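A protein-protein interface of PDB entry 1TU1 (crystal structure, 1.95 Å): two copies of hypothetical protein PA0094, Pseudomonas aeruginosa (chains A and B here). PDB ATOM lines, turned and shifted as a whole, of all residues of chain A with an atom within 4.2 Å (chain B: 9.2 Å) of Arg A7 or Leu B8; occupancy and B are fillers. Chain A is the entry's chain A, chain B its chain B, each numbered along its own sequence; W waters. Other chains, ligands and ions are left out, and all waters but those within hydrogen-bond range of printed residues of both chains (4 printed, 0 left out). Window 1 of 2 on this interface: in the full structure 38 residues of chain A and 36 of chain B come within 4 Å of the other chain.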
ATOM      1  N   LEU A   5      11.023  14.032 -31.417  1.00  0.00           N
ATOM      2  CA  LEU A   5      10.585  12.657 -31.635  1.00  0.00           C
ATOM      3  C   LEU A   5       9.698  12.161 -30.500  1.00  0.00           C
ATOM      4  O   LEU A   5      10.135  12.095 -29.365  1.00  0.00           O
ATOM      5  CB  LEU A   5      11.788  11.725 -31.760  1.00  0.00           C
ATOM      6  CG  LEU A   5      11.504  10.347 -32.355  1.00  0.00           C
ATOM      7  CD1 LEU A   5      10.690  10.414 -33.645  1.00  0.00           C
ATOM      8  CD2 LEU A   5      12.842   9.631 -32.615  1.00  0.00           C
ATOM      9  N   TYR A   6       8.468  11.787 -30.815  1.00  0.00           N
ATOM     10  CA  TYR A   6       7.497  11.374 -29.817  1.00  0.00           C
ATOM     11  C   TYR A   6       7.214   9.873 -29.966  1.00  0.00           C
ATOM     12  O   TYR A   6       6.919   9.390 -31.052  1.00  0.00           O
ATOM     13  CB  TYR A   6       6.215  12.163 -30.016  1.00  0.00           C
ATOM     14  CG  TYR A   6       5.179  11.849 -28.990  1.00  0.00           C
ATOM     15  CD1 TYR A   6       5.187  12.487 -27.754  1.00  0.00           C
ATOM     16  CD2 TYR A   6       4.174  10.892 -29.243  1.00  0.00           C
ATOM     17  CE1 TYR A   6       4.241  12.186 -26.797  1.00  0.00           C
ATOM     18  CE2 TYR A   6       3.219  10.606 -28.292  1.00  0.00           C
ATOM     19  CZ  TYR A   6       3.262  11.239 -27.065  1.00  0.00           C
ATOM     20  OH  TYR A   6       2.310  10.946 -26.113  1.00  0.00           O
ATOM     21  N   ARG A   7       7.300   9.157 -28.865  1.00  0.00           N
ATOM     22  CA  ARG A   7       7.181   7.713 -28.859  1.00  0.00           C
ATOM     23  C   ARG A   7       5.811   7.303 -28.314  1.00  0.00           C
ATOM     24  O   ARG A   7       5.378   7.769 -27.235  1.00  0.00           O
ATOM     25  CB  ARG A   7       8.283   7.039 -28.021  1.00  0.00           C
ATOM     26  CG  ARG A   7       9.641   7.706 -28.064  1.00  0.00           C
ATOM     27  CD  ARG A   7      10.151   8.046 -29.456  1.00  0.00           C
ATOM     28  NE  ARG A   7      11.585   8.347 -29.575  1.00  0.00           N
ATOM     29  CZ  ARG A   7      12.347   9.029 -28.712  1.00  0.00           C
ATOM     30  NH1 ARG A   7      11.874   9.518 -27.568  1.00  0.00           N
ATOM     31  NH2 ARG A   7      13.634   9.216 -29.006  1.00  0.00           N
ATOM     32  N   LEU A   8       5.118   6.464 -29.091  1.00  0.00           N
ATOM     33  CA  LEU A   8       3.941   5.746 -28.619  1.00  0.00           C
ATOM     34  C   LEU A   8       4.129   4.236 -28.864  1.00  0.00           C
ATOM     35  O   LEU A   8       5.156   3.799 -29.377  1.00  0.00           O
ATOM     36  CB  LEU A   8       2.657   6.282 -29.252  1.00  0.00           C
ATOM     37  CG  LEU A   8       2.536   6.411 -30.769  1.00  0.00           C
ATOM     38  CD1 LEU A   8       1.089   6.284 -31.192  1.00  0.00           C
ATOM     39  CD2 LEU A   8       3.103   7.726 -31.268  1.00  0.00           C
ATOM     40  N   ALA A  11       4.005   3.351 -32.737  1.00  0.00           N
ATOM     41  CA  ALA A  11       4.714   4.170 -33.708  1.00  0.00           C
ATOM     42  C   ALA A  11       5.588   5.252 -33.048  1.00  0.00           C
ATOM     43  O   ALA A  11       5.517   5.469 -31.845  1.00  0.00           O
ATOM     44  CB  ALA A  11       3.700   4.858 -34.608  1.00  0.00           C
ATOM     45  N   ASP A  12       6.393   5.921 -33.870  1.00  0.00           N
ATOM     46  CA  ASP A  12       7.095   7.146 -33.494  1.00  0.00           C
ATOM     47  C   ASP A  12       6.786   8.181 -34.528  1.00  0.00           C
ATOM     48  O   ASP A  12       6.583   7.850 -35.687  1.00  0.00           O
ATOM     49  CB  ASP A  12       8.595   6.910 -33.465  1.00  0.00           C
ATOM     50  CG  ASP A  12       8.956   5.795 -32.566  1.00  0.00           C
ATOM     51  OD1 ASP A  12       9.044   6.041 -31.352  1.00  0.00           O
ATOM     52  OD2 ASP A  12       9.059   4.612 -32.969  1.00  0.00           O
ATOM     53  N   ASN A  25      -3.273   7.601 -21.568  1.00  0.00           N
ATOM     54  CA  ASN A  25      -3.310   6.150 -21.733  1.00  0.00           C
ATOM     55  C   ASN A  25      -4.376   5.581 -20.836  1.00  0.00           C
ATOM     56  O   ASN A  25      -4.447   5.926 -19.658  1.00  0.00           O
ATOM     57  CB  ASN A  25      -1.975   5.506 -21.445  1.00  0.00           C
ATOM     58  CG  ASN A  25      -0.874   6.052 -22.320  1.00  0.00           C
ATOM     59  OD1 ASN A  25      -0.729   5.661 -23.491  1.00  0.00           O
ATOM     60  ND2 ASN A  25      -0.127   7.015 -21.783  1.00  0.00           N
ATOM     61  N   ILE A  42      -3.067   6.889 -17.411  1.00  0.00           N
ATOM     62  CA  ILE A  42      -1.829   7.670 -17.360  1.00  0.00           C
ATOM     63  C   ILE A  42      -2.086   8.981 -18.045  1.00  0.00           C
ATOM     64  O   ILE A  42      -2.515   9.003 -19.227  1.00  0.00           O
ATOM     65  CB  ILE A  42      -0.689   6.938 -18.042  1.00  0.00           C
ATOM     66  CG1 ILE A  42      -0.562   5.508 -17.486  1.00  0.00           C
ATOM     67  CG2 ILE A  42       0.646   7.722 -17.847  1.00  0.00           C
ATOM     68  CD1 ILE A  42       0.455   4.669 -18.241  1.00  0.00           C
ATOM     69  N   ARG A  44      -0.675  13.440 -18.078  1.00  0.00           N
ATOM     70  CA  ARG A  44       0.477  14.344 -17.977  1.00  0.00           C
ATOM     71  C   ARG A  44       0.008  15.696 -17.459  1.00  0.00           C
ATOM     72  O   ARG A  44      -1.091  16.154 -17.793  1.00  0.00           O
ATOM     73  CB  ARG A  44       1.120  14.592 -19.345  1.00  0.00           C
ATOM     74  CG  ARG A  44       1.755  13.387 -19.984  1.00  0.00           C
ATOM     75  CD  ARG A  44       0.771  12.567 -20.828  1.00  0.00           C
ATOM     76  NE  ARG A  44       1.426  11.380 -21.339  1.00  0.00           N
ATOM     77  CZ  ARG A  44       0.891  10.185 -21.519  1.00  0.00           C
ATOM     78  NH1 ARG A  44      -0.375   9.948 -21.205  1.00  0.00           N
ATOM     79  NH2 ARG A  44       1.680   9.217 -22.009  1.00  0.00           N
ATOM     80  N   ARG A 142      11.344   7.018 -18.569  1.00  0.00           N
ATOM     81  CA  ARG A 142      12.310   7.160 -19.643  1.00  0.00           C
ATOM     82  C   ARG A 142      13.097   8.463 -19.436  1.00  0.00           C
ATOM     83  O   ARG A 142      12.510   9.503 -19.143  1.00  0.00           O
ATOM     84  CB  ARG A 142      11.596   7.194 -20.990  1.00  0.00           C
ATOM     85  CG  ARG A 142      12.517   7.190 -22.203  1.00  0.00           C
ATOM     86  CD  ARG A 142      11.795   7.178 -23.556  1.00  0.00           C
ATOM     87  NE  ARG A 142      11.394   5.828 -23.968  1.00  0.00           N
ATOM     88  CZ  ARG A 142      10.268   5.213 -23.601  1.00  0.00           C
ATOM     89  NH1 ARG A 142       9.390   5.804 -22.811  1.00  0.00           N
ATOM     90  NH2 ARG A 142      10.006   3.989 -24.030  1.00  0.00           N
ATOM     91  N   LEU B   5       5.143  -5.617 -22.468  1.00  0.00           N
ATOM     92  CA  LEU B   5       5.786  -4.341 -22.173  1.00  0.00           C
ATOM     93  C   LEU B   5       5.086  -3.293 -23.012  1.00  0.00           C
ATOM     94  O   LEU B   5       4.978  -3.444 -24.233  1.00  0.00           O
ATOM     95  CB  LEU B   5       7.271  -4.397 -22.525  1.00  0.00           C
ATOM     96  CG  LEU B   5       8.132  -3.236 -21.992  1.00  0.00           C
ATOM     97  CD1 LEU B   5       8.120  -3.190 -20.479  1.00  0.00           C
ATOM     98  CD2 LEU B   5       9.559  -3.389 -22.505  1.00  0.00           C
ATOM     99  N   TYR B   6       4.573  -2.252 -22.374  1.00  0.00           N
ATOM    100  CA  TYR B   6       3.880  -1.193 -23.087  1.00  0.00           C
ATOM    101  C   TYR B   6       4.766   0.042 -23.107  1.00  0.00           C
ATOM    102  O   TYR B   6       5.285   0.454 -22.069  1.00  0.00           O
ATOM    103  CB  TYR B   6       2.552  -0.882 -22.395  1.00  0.00           C
ATOM    104  CG  TYR B   6       1.732   0.140 -23.111  1.00  0.00           C
ATOM    105  CD1 TYR B   6       0.876  -0.217 -24.150  1.00  0.00           C
ATOM    106  CD2 TYR B   6       1.804   1.483 -22.758  1.00  0.00           C
ATOM    107  CE1 TYR B   6       0.127   0.757 -24.821  1.00  0.00           C
ATOM    108  CE2 TYR B   6       1.069   2.435 -23.415  1.00  0.00           C
ATOM    109  CZ  TYR B   6       0.227   2.076 -24.450  1.00  0.00           C
ATOM    110  OH  TYR B   6      -0.474   3.048 -25.137  1.00  0.00           O
ATOM    111  N   ARG B   7       4.886   0.657 -24.276  1.00  0.00           N
ATOM    112  CA  ARG B   7       5.741   1.810 -24.465  1.00  0.00           C
ATOM    113  C   ARG B   7       4.906   3.099 -24.577  1.00  0.00           C
ATOM    114  O   ARG B   7       3.907   3.181 -25.325  1.00  0.00           O
ATOM    115  CB  ARG B   7       6.588   1.581 -25.724  1.00  0.00           C
ATOM    116  CG  ARG B   7       7.562   2.672 -26.079  1.00  0.00           C
ATOM    117  CD  ARG B   7       8.478   2.305 -27.263  1.00  0.00           C
ATOM    118  NE  ARG B   7       7.797   2.525 -28.539  1.00  0.00           N
ATOM    119  CZ  ARG B   7       8.289   3.194 -29.587  1.00  0.00           C
ATOM    120  NH1 ARG B   7       9.507   3.728 -29.561  1.00  0.00           N
ATOM    121  NH2 ARG B   7       7.545   3.330 -30.676  1.00  0.00           N
ATOM    122  N   LEU B   8       5.294   4.082 -23.762  1.00  0.00           N
ATOM    123  CA  LEU B   8       4.786   5.432 -23.872  1.00  0.00           C
ATOM    124  C   LEU B   8       5.972   6.402 -23.902  1.00  0.00           C
ATOM    125  O   LEU B   8       7.124   6.004 -23.769  1.00  0.00           O
ATOM    126  CB  LEU B   8       3.775   5.758 -22.783  1.00  0.00           C
ATOM    127  CG  LEU B   8       4.124   5.536 -21.323  1.00  0.00           C
ATOM    128  CD1 LEU B   8       3.402   6.601 -20.466  1.00  0.00           C
ATOM    129  CD2 LEU B   8       3.754   4.134 -20.876  1.00  0.00           C
ATOM    130  N   HIS B   9       5.705   7.659 -24.162  1.00  0.00           N
ATOM    131  CA  HIS B   9       6.796   8.583 -24.445  1.00  0.00           C
ATOM    132  C   HIS B   9       7.654   8.762 -23.193  1.00  0.00           C
ATOM    133  O   HIS B   9       8.867   8.879 -23.278  1.00  0.00           O
ATOM    134  CB  HIS B   9       6.248   9.925 -24.923  1.00  0.00           C
ATOM    135  CG  HIS B   9       7.304  10.923 -25.273  1.00  0.00           C
ATOM    136  ND1 HIS B   9       8.133  10.780 -26.368  1.00  0.00           N
ATOM    137  CD2 HIS B   9       7.649  12.099 -24.685  1.00  0.00           C
ATOM    138  CE1 HIS B   9       8.951  11.823 -26.434  1.00  0.00           C
ATOM    139  NE2 HIS B   9       8.680  12.635 -25.422  1.00  0.00           N
ATOM    140  N   GLU B  10       6.999   8.729 -22.040  1.00  0.00           N
ATOM    141  CA  GLU B  10       7.614   9.053 -20.750  1.00  0.00           C
ATOM    142  C   GLU B  10       8.068   7.860 -19.925  1.00  0.00           C
ATOM    143  O   GLU B  10       8.692   8.042 -18.866  1.00  0.00           O
ATOM    144  CB  GLU B  10       6.626   9.845 -19.902  1.00  0.00           C
ATOM    145  CG  GLU B  10       6.135  11.131 -20.534  1.00  0.00           C
ATOM    146  CD  GLU B  10       4.933  10.967 -21.439  1.00  0.00           C
ATOM    147  OE1 GLU B  10       4.458   9.819 -21.657  1.00  0.00           O
ATOM    148  OE2 GLU B  10       4.471  11.992 -21.961  1.00  0.00           O
ATOM    149  N   ALA B  11       7.748   6.646 -20.372  1.00  0.00           N
ATOM    150  CA  ALA B  11       8.006   5.456 -19.571  1.00  0.00           C
ATOM    151  C   ALA B  11       7.720   4.159 -20.323  1.00  0.00           C
ATOM    152  O   ALA B  11       7.150   4.177 -21.400  1.00  0.00           O
ATOM    153  CB  ALA B  11       7.163   5.480 -18.350  1.00  0.00           C
ATOM    154  N   ASP B  12       8.136   3.051 -19.721  1.00  0.00           N
ATOM    155  CA  ASP B  12       7.689   1.700 -20.104  1.00  0.00           C
ATOM    156  C   ASP B  12       7.139   1.040 -18.866  1.00  0.00           C
ATOM    157  O   ASP B  12       7.565   1.353 -17.765  1.00  0.00           O
ATOM    158  CB  ASP B  12       8.855   0.862 -20.630  1.00  0.00           C
ATOM    159  CG  ASP B  12       9.477   1.457 -21.847  1.00  0.00           C
ATOM    160  OD1 ASP B  12       8.821   1.453 -22.907  1.00  0.00           O
ATOM    161  OD2 ASP B  12      10.600   1.983 -21.841  1.00  0.00           O
ATOM    162  N   LEU B  13       6.148   0.162 -19.034  1.00  0.00           N
ATOM    163  CA  LEU B  13       5.681  -0.685 -17.945  1.00  0.00           C
ATOM    164  C   LEU B  13       5.050  -1.955 -18.520  1.00  0.00           C
ATOM    165  O   LEU B  13       4.704  -2.011 -19.705  1.00  0.00           O
ATOM    166  CB  LEU B  13       4.700   0.042 -17.026  1.00  0.00           C
ATOM    167  CG  LEU B  13       3.246   0.204 -17.479  1.00  0.00           C
ATOM    168  CD1 LEU B  13       2.370   0.655 -16.353  1.00  0.00           C
ATOM    169  CD2 LEU B  13       3.160   1.154 -18.661  1.00  0.00           C
ATOM    170  N   GLU B  14       4.945  -2.983 -17.693  1.00  0.00           N
ATOM    171  CA  GLU B  14       4.282  -4.229 -18.115  1.00  0.00           C
ATOM    172  C   GLU B  14       2.795  -4.136 -17.876  1.00  0.00           C
ATOM    173  O   GLU B  14       2.359  -3.884 -16.762  1.00  0.00           O
ATOM    174  CB  GLU B  14       4.882  -5.412 -17.378  1.00  0.00           C
ATOM    175  CG  GLU B  14       6.289  -5.693 -17.847  1.00  0.00           C
ATOM    176  CD  GLU B  14       6.958  -6.856 -17.122  1.00  0.00           C
ATOM    177  OE1 GLU B  14       6.386  -7.434 -16.164  1.00  0.00           O
ATOM    178  OE2 GLU B  14       8.083  -7.166 -17.522  1.00  0.00           O
ATOM    179  N   ILE B  15       2.019  -4.324 -18.940  1.00  0.00           N
ATOM    180  CA  ILE B  15       0.570  -4.288 -18.873  1.00  0.00           C
ATOM    181  C   ILE B  15       0.018  -5.712 -19.109  1.00  0.00           C
ATOM    182  O   ILE B  15       0.346  -6.337 -20.112  1.00  0.00           O
ATOM    183  CB  ILE B  15       0.020  -3.322 -19.957  1.00  0.00           C
ATOM    184  CG1 ILE B  15       0.467  -1.872 -19.675  1.00  0.00           C
ATOM    185  CG2 ILE B  15      -1.526  -3.409 -20.067  1.00  0.00           C
ATOM    186  CD1 ILE B  15      -0.224  -1.236 -18.504  1.00  0.00           C
ATOM    187  N   SER B  23      -6.213   3.860 -25.122  1.00  0.00           N
ATOM    188  CA  SER B  23      -5.320   5.007 -25.075  1.00  0.00           C
ATOM    189  C   SER B  23      -5.526   5.954 -26.254  1.00  0.00           C
ATOM    190  O   SER B  23      -5.845   5.544 -27.378  1.00  0.00           O
ATOM    191  CB  SER B  23      -3.859   4.552 -25.035  1.00  0.00           C
ATOM    192  OG  SER B  23      -3.619   3.780 -23.851  1.00  0.00           O
ATOM    193  N   ASN B  25      -3.689   9.627 -27.866  1.00  0.00           N
ATOM    194  CA  ASN B  25      -2.758  10.755 -27.874  1.00  0.00           C
ATOM    195  C   ASN B  25      -3.462  11.982 -28.432  1.00  0.00           C
ATOM    196  O   ASN B  25      -4.225  11.894 -29.421  1.00  0.00           O
ATOM    197  CB  ASN B  25      -1.487  10.420 -28.634  1.00  0.00           C
ATOM    198  CG  ASN B  25      -0.795   9.191 -28.086  1.00  0.00           C
ATOM    199  OD1 ASN B  25      -0.021   9.242 -27.104  1.00  0.00           O
ATOM    200  ND2 ASN B  25      -1.081   8.063 -28.701  1.00  0.00           N
ATOM    201  N   PHE B  27      -3.035  16.270 -29.095  1.00  0.00           N
ATOM    202  CA  PHE B  27      -2.148  17.421 -29.233  1.00  0.00           C
ATOM    203  C   PHE B  27      -2.990  18.625 -29.667  1.00  0.00           C
ATOM    204  O   PHE B  27      -3.795  18.536 -30.591  1.00  0.00           O
ATOM    205  CB  PHE B  27      -1.042  17.145 -30.246  1.00  0.00           C
ATOM    206  CG  PHE B  27      -0.123  16.024 -29.855  1.00  0.00           C
ATOM    207  CD1 PHE B  27       0.971  16.265 -29.043  1.00  0.00           C
ATOM    208  CD2 PHE B  27      -0.345  14.724 -30.303  1.00  0.00           C
ATOM    209  CE1 PHE B  27       1.812  15.232 -28.667  1.00  0.00           C
ATOM    210  CE2 PHE B  27       0.480  13.685 -29.901  1.00  0.00           C
ATOM    211  CZ  PHE B  27       1.564  13.941 -29.099  1.00  0.00           C
ATOM    212  N   ILE B  42      -4.396  10.807 -32.011  1.00  0.00           N
ATOM    213  CA  ILE B  42      -4.055   9.467 -32.454  1.00  0.00           C
ATOM    214  C   ILE B  42      -4.881   8.517 -31.616  1.00  0.00           C
ATOM    215  O   ILE B  42      -4.779   8.511 -30.373  1.00  0.00           O
ATOM    216  CB  ILE B  42      -2.572   9.143 -32.268  1.00  0.00           C
ATOM    217  CG1 ILE B  42      -1.676  10.235 -32.871  1.00  0.00           C
ATOM    218  CG2 ILE B  42      -2.232   7.741 -32.838  1.00  0.00           C
ATOM    219  CD1 ILE B  42      -0.186   9.974 -32.630  1.00  0.00           C
ATOM    220  N   ARG B  44      -6.973   4.351 -31.596  1.00  0.00           N
ATOM    221  CA  ARG B  44      -6.801   2.955 -32.018  1.00  0.00           C
ATOM    222  C   ARG B  44      -8.175   2.348 -32.226  1.00  0.00           C
ATOM    223  O   ARG B  44      -9.089   2.646 -31.478  1.00  0.00           O
ATOM    224  CB  ARG B  44      -6.094   2.141 -30.947  1.00  0.00           C
ATOM    225  CG  ARG B  44      -4.619   2.488 -30.756  1.00  0.00           C
ATOM    226  CD  ARG B  44      -4.447   3.742 -29.881  1.00  0.00           C
ATOM    227  NE  ARG B  44      -3.070   3.938 -29.461  1.00  0.00           N
ATOM    228  CZ  ARG B  44      -2.563   5.113 -29.099  1.00  0.00           C
ATOM    229  NH1 ARG B  44      -3.316   6.213 -29.094  1.00  0.00           N
ATOM    230  NH2 ARG B  44      -1.296   5.174 -28.770  1.00  0.00           N
ATOM    231  N   VAL B 140       6.385   6.686 -38.252  1.00  0.00           N
ATOM    232  CA  VAL B 140       6.862   5.344 -38.566  1.00  0.00           C
ATOM    233  C   VAL B 140       6.193   4.297 -37.671  1.00  0.00           C
ATOM    234  O   VAL B 140       6.468   4.221 -36.477  1.00  0.00           O
ATOM    235  CB  VAL B 140       8.402   5.263 -38.381  1.00  0.00           C
ATOM    236  CG1 VAL B 140       8.917   3.842 -38.716  1.00  0.00           C
ATOM    237  CG2 VAL B 140       9.101   6.321 -39.257  1.00  0.00           C
ATOM    238  N   ARG B 142       5.473   1.011 -35.679  1.00  0.00           N
ATOM    239  CA  ARG B 142       6.337   0.035 -35.059  1.00  0.00           C
ATOM    240  C   ARG B 142       5.872  -1.334 -35.554  1.00  0.00           C
ATOM    241  O   ARG B 142       4.673  -1.562 -35.713  1.00  0.00           O
ATOM    242  CB  ARG B 142       6.225   0.128 -33.543  1.00  0.00           C
ATOM    243  CG  ARG B 142       7.075  -0.859 -32.770  1.00  0.00           C
ATOM    244  CD  ARG B 142       7.201  -0.540 -31.289  1.00  0.00           C
ATOM    245  NE  ARG B 142       8.282   0.427 -31.099  1.00  0.00           N
ATOM    246  CZ  ARG B 142       9.525   0.118 -30.725  1.00  0.00           C
ATOM    247  NH1 ARG B 142       9.887  -1.143 -30.476  1.00  0.00           N
ATOM    248  NH2 ARG B 142      10.427   1.083 -30.609  1.00  0.00           N
HETATM  249  O   HOH W   1       2.668  12.183 -23.987  1.00  0.00           O
HETATM  250  O   HOH W   2       3.346   8.215 -25.629  1.00  0.00           O
HETATM  251  O   HOH W   3       1.010   6.980 -25.577  1.00  0.00           O
HETATM  252  O   HOH W   4       8.780   3.380 -35.224  1.00  0.00           O
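O of Arg A7 lies within hydrogen-bond range of N of His B9 (3.1 Å). The side-chain carboxylate (OD1) of Asp B12 is in salt-bridge range of the guanidinium group (NH2) of Arg A142 (3.0 Å). N of Arg A142 is in hydrogen-bond range of O of Glu B10 (2.9 Å). O of Asp A12 sits at hydrogen-bond distance from N of Val B140. O of Ala B11 is in hydrogen-bond range of NH1 of Arg A142, 3.1 Å away. OE1 of Glu B10 is in salt-bridge range of NH2 of Arg A44 (2.9 Å). The side-chain hydroxyl of Tyr B6 lies within hydrogen-bond range of the side-chain amide oxygen of Asn A25 (3.1 Å). OG of Ser B23 lies close to OD1 of Asn A25 (3.5 Å). The backbone carbonyl oxygen (O) of Ala A11 is in hydrogen-bond range of the guanidinium group (NH2) of Arg B7 (3.2 Å). NH1 of Arg A142 is in hydrogen-bond range of O of Leu B8 (2.5 Å). OD1 of Asp A12 is in salt-bridge range of NH1 of Arg B7, at 3.0 Å. O of Leu A8 lies within hydrogen-bond range of NH2 of Arg B7 (2.8 Å). OD1 of Asn B25 lies within hydrogen-bond range of OH of Tyr A6 (3.1 Å). The guanidinium group (NH1) of Arg A142 lies within hydrogen-bond range of the backbone carbonyl oxygen (O) of His B9, at 3.2 Å.
O of Leu B13 sits at hydrogen-bond distance from N of Tyr B6 (2.7 Å). NE of Arg A7 is in salt-bridge range of OD1 of Asp A12 (3.9 Å). O of Ser B23 is in hydrogen-bond range of NH1 of Arg B44, 3.1 Å away. ND2 of Asn A25 lies close to NH2 of Arg A44 (2.9 Å). OG of Ser B23 sits at hydrogen-bond distance from OH of Tyr B6 (3.5 Å). The backbone carbonyl oxygen of Asn A25 is in hydrogen-bond range of the backbone NH of Ile A42 (2.8 Å).
Among the printed residues, merely in contact across the chains: Leu A5 with His B9, Tyr A6 with His B9, Tyr A6 with Phe B27, Arg A7 with Arg B7, Arg A7 with Leu B8, Leu A8 with Asn B25, Leu A8 with Ile B42, Leu A8 with Arg B44, Ala A11 with Val B140, Ala A11 with Arg B142, Asn A25 with Leu B8, Ile A42 with Leu B8, Arg A44 with Leu B8 and Arg A142 with Arg B7.
Of the printed residues of chain B, Arg A7 touches Arg B7, Leu B8 and His B9. Of the printed residues of chain A, Leu B8 touches Arg A7 (3.7 Å), Asn A25 (3.8 Å), Ile A42 (3.96 Å), Arg A44 (3.5 Å) and Arg A142 (2.5 Å). Tyr A6 touches three residues of chain B. Printed residues of chain A within 4 Å of Val B140: Ala A11 and Asp A12. Printed residues of chain A within 4 Å of Asn B25: Tyr A6 and Leu A8. Of the printed residues of chain A, Phe B27 touches Tyr A6 (3.8 Å). Of the printed residues of chain A, His B9 touches Leu A5, Tyr A6, Arg A7 and Arg A142. Printed residues of chain A within 4 Å of Ser B23: Asn A25. Leu B5 touches none of the printed residues of chain A. Leu B13 touches none of the printed residues of chain A. The nearest printed residue of chain B that does not touch Arg A7 is Glu B10 (5.5 Å). The nearest printed residue of chain A that does not touch Leu B8 is Leu A8 (4.8 Å).
Of the 10 printed residues of chain A, 10 touch a printed residue of chain B. Printed residues of chain A that touch a printed residue of chain B: Leu A5, Tyr A6, Arg A7, Leu A8, Ala A11, Asp A12, Asn A25, Ile A42, Arg A44 and Arg A142. Hydrophobic or aromatic side chains of chain A that line the printed part of chain B: Tyr A6, Leu A8, Ala A11 and Ile A42. Among the printed residues, 28 pairs touch across the chains.
Tyr A6 touches Asn B25, and with the chains exchanged Asn A25 touches Tyr B6. Leu A8 touches Asn B25, and with the chains exchanged Asn A25 touches Leu B8. Asp A12 touches Arg B7, but with the chains exchanged Arg A7 does not touch Asp B12 (7.6 Å). Arg A142 touches Asp B12, but with the chains exchanged Asp A12 does not touch Arg B142 (4.5 Å). Of the 28 pairs that touch across the chains among the printed residues, 13 have their exchanged pair printed and touching as well.
Water W1 lies within hydrogen-bond range of the side-chain hydroxyl (OH) of Tyr A6, the side-chain carboxylate (OE2) of Glu B10 and the guanidinium group (NE) of Arg A44. Water W4 bridges the side-chain carboxylate (OD2) of Asp A12 (2.6 Å) and the backbone carbonyl oxygen (O) of Val B140 (2.8 Å). Water W2 lies within hydrogen-bond range of the backbone carbonyl oxygen (O) of Arg A7 (2.6 Å), the backbone NH (N) of His B9 (2.8 Å) and the side-chain hydroxyl (OH) of Tyr A6 (3.0 Å). Water W3 bridges the side-chain amide oxygen of Asn B25 (2.9 Å) and the side-chain amide oxygen of Asn A25 (3.0 Å).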
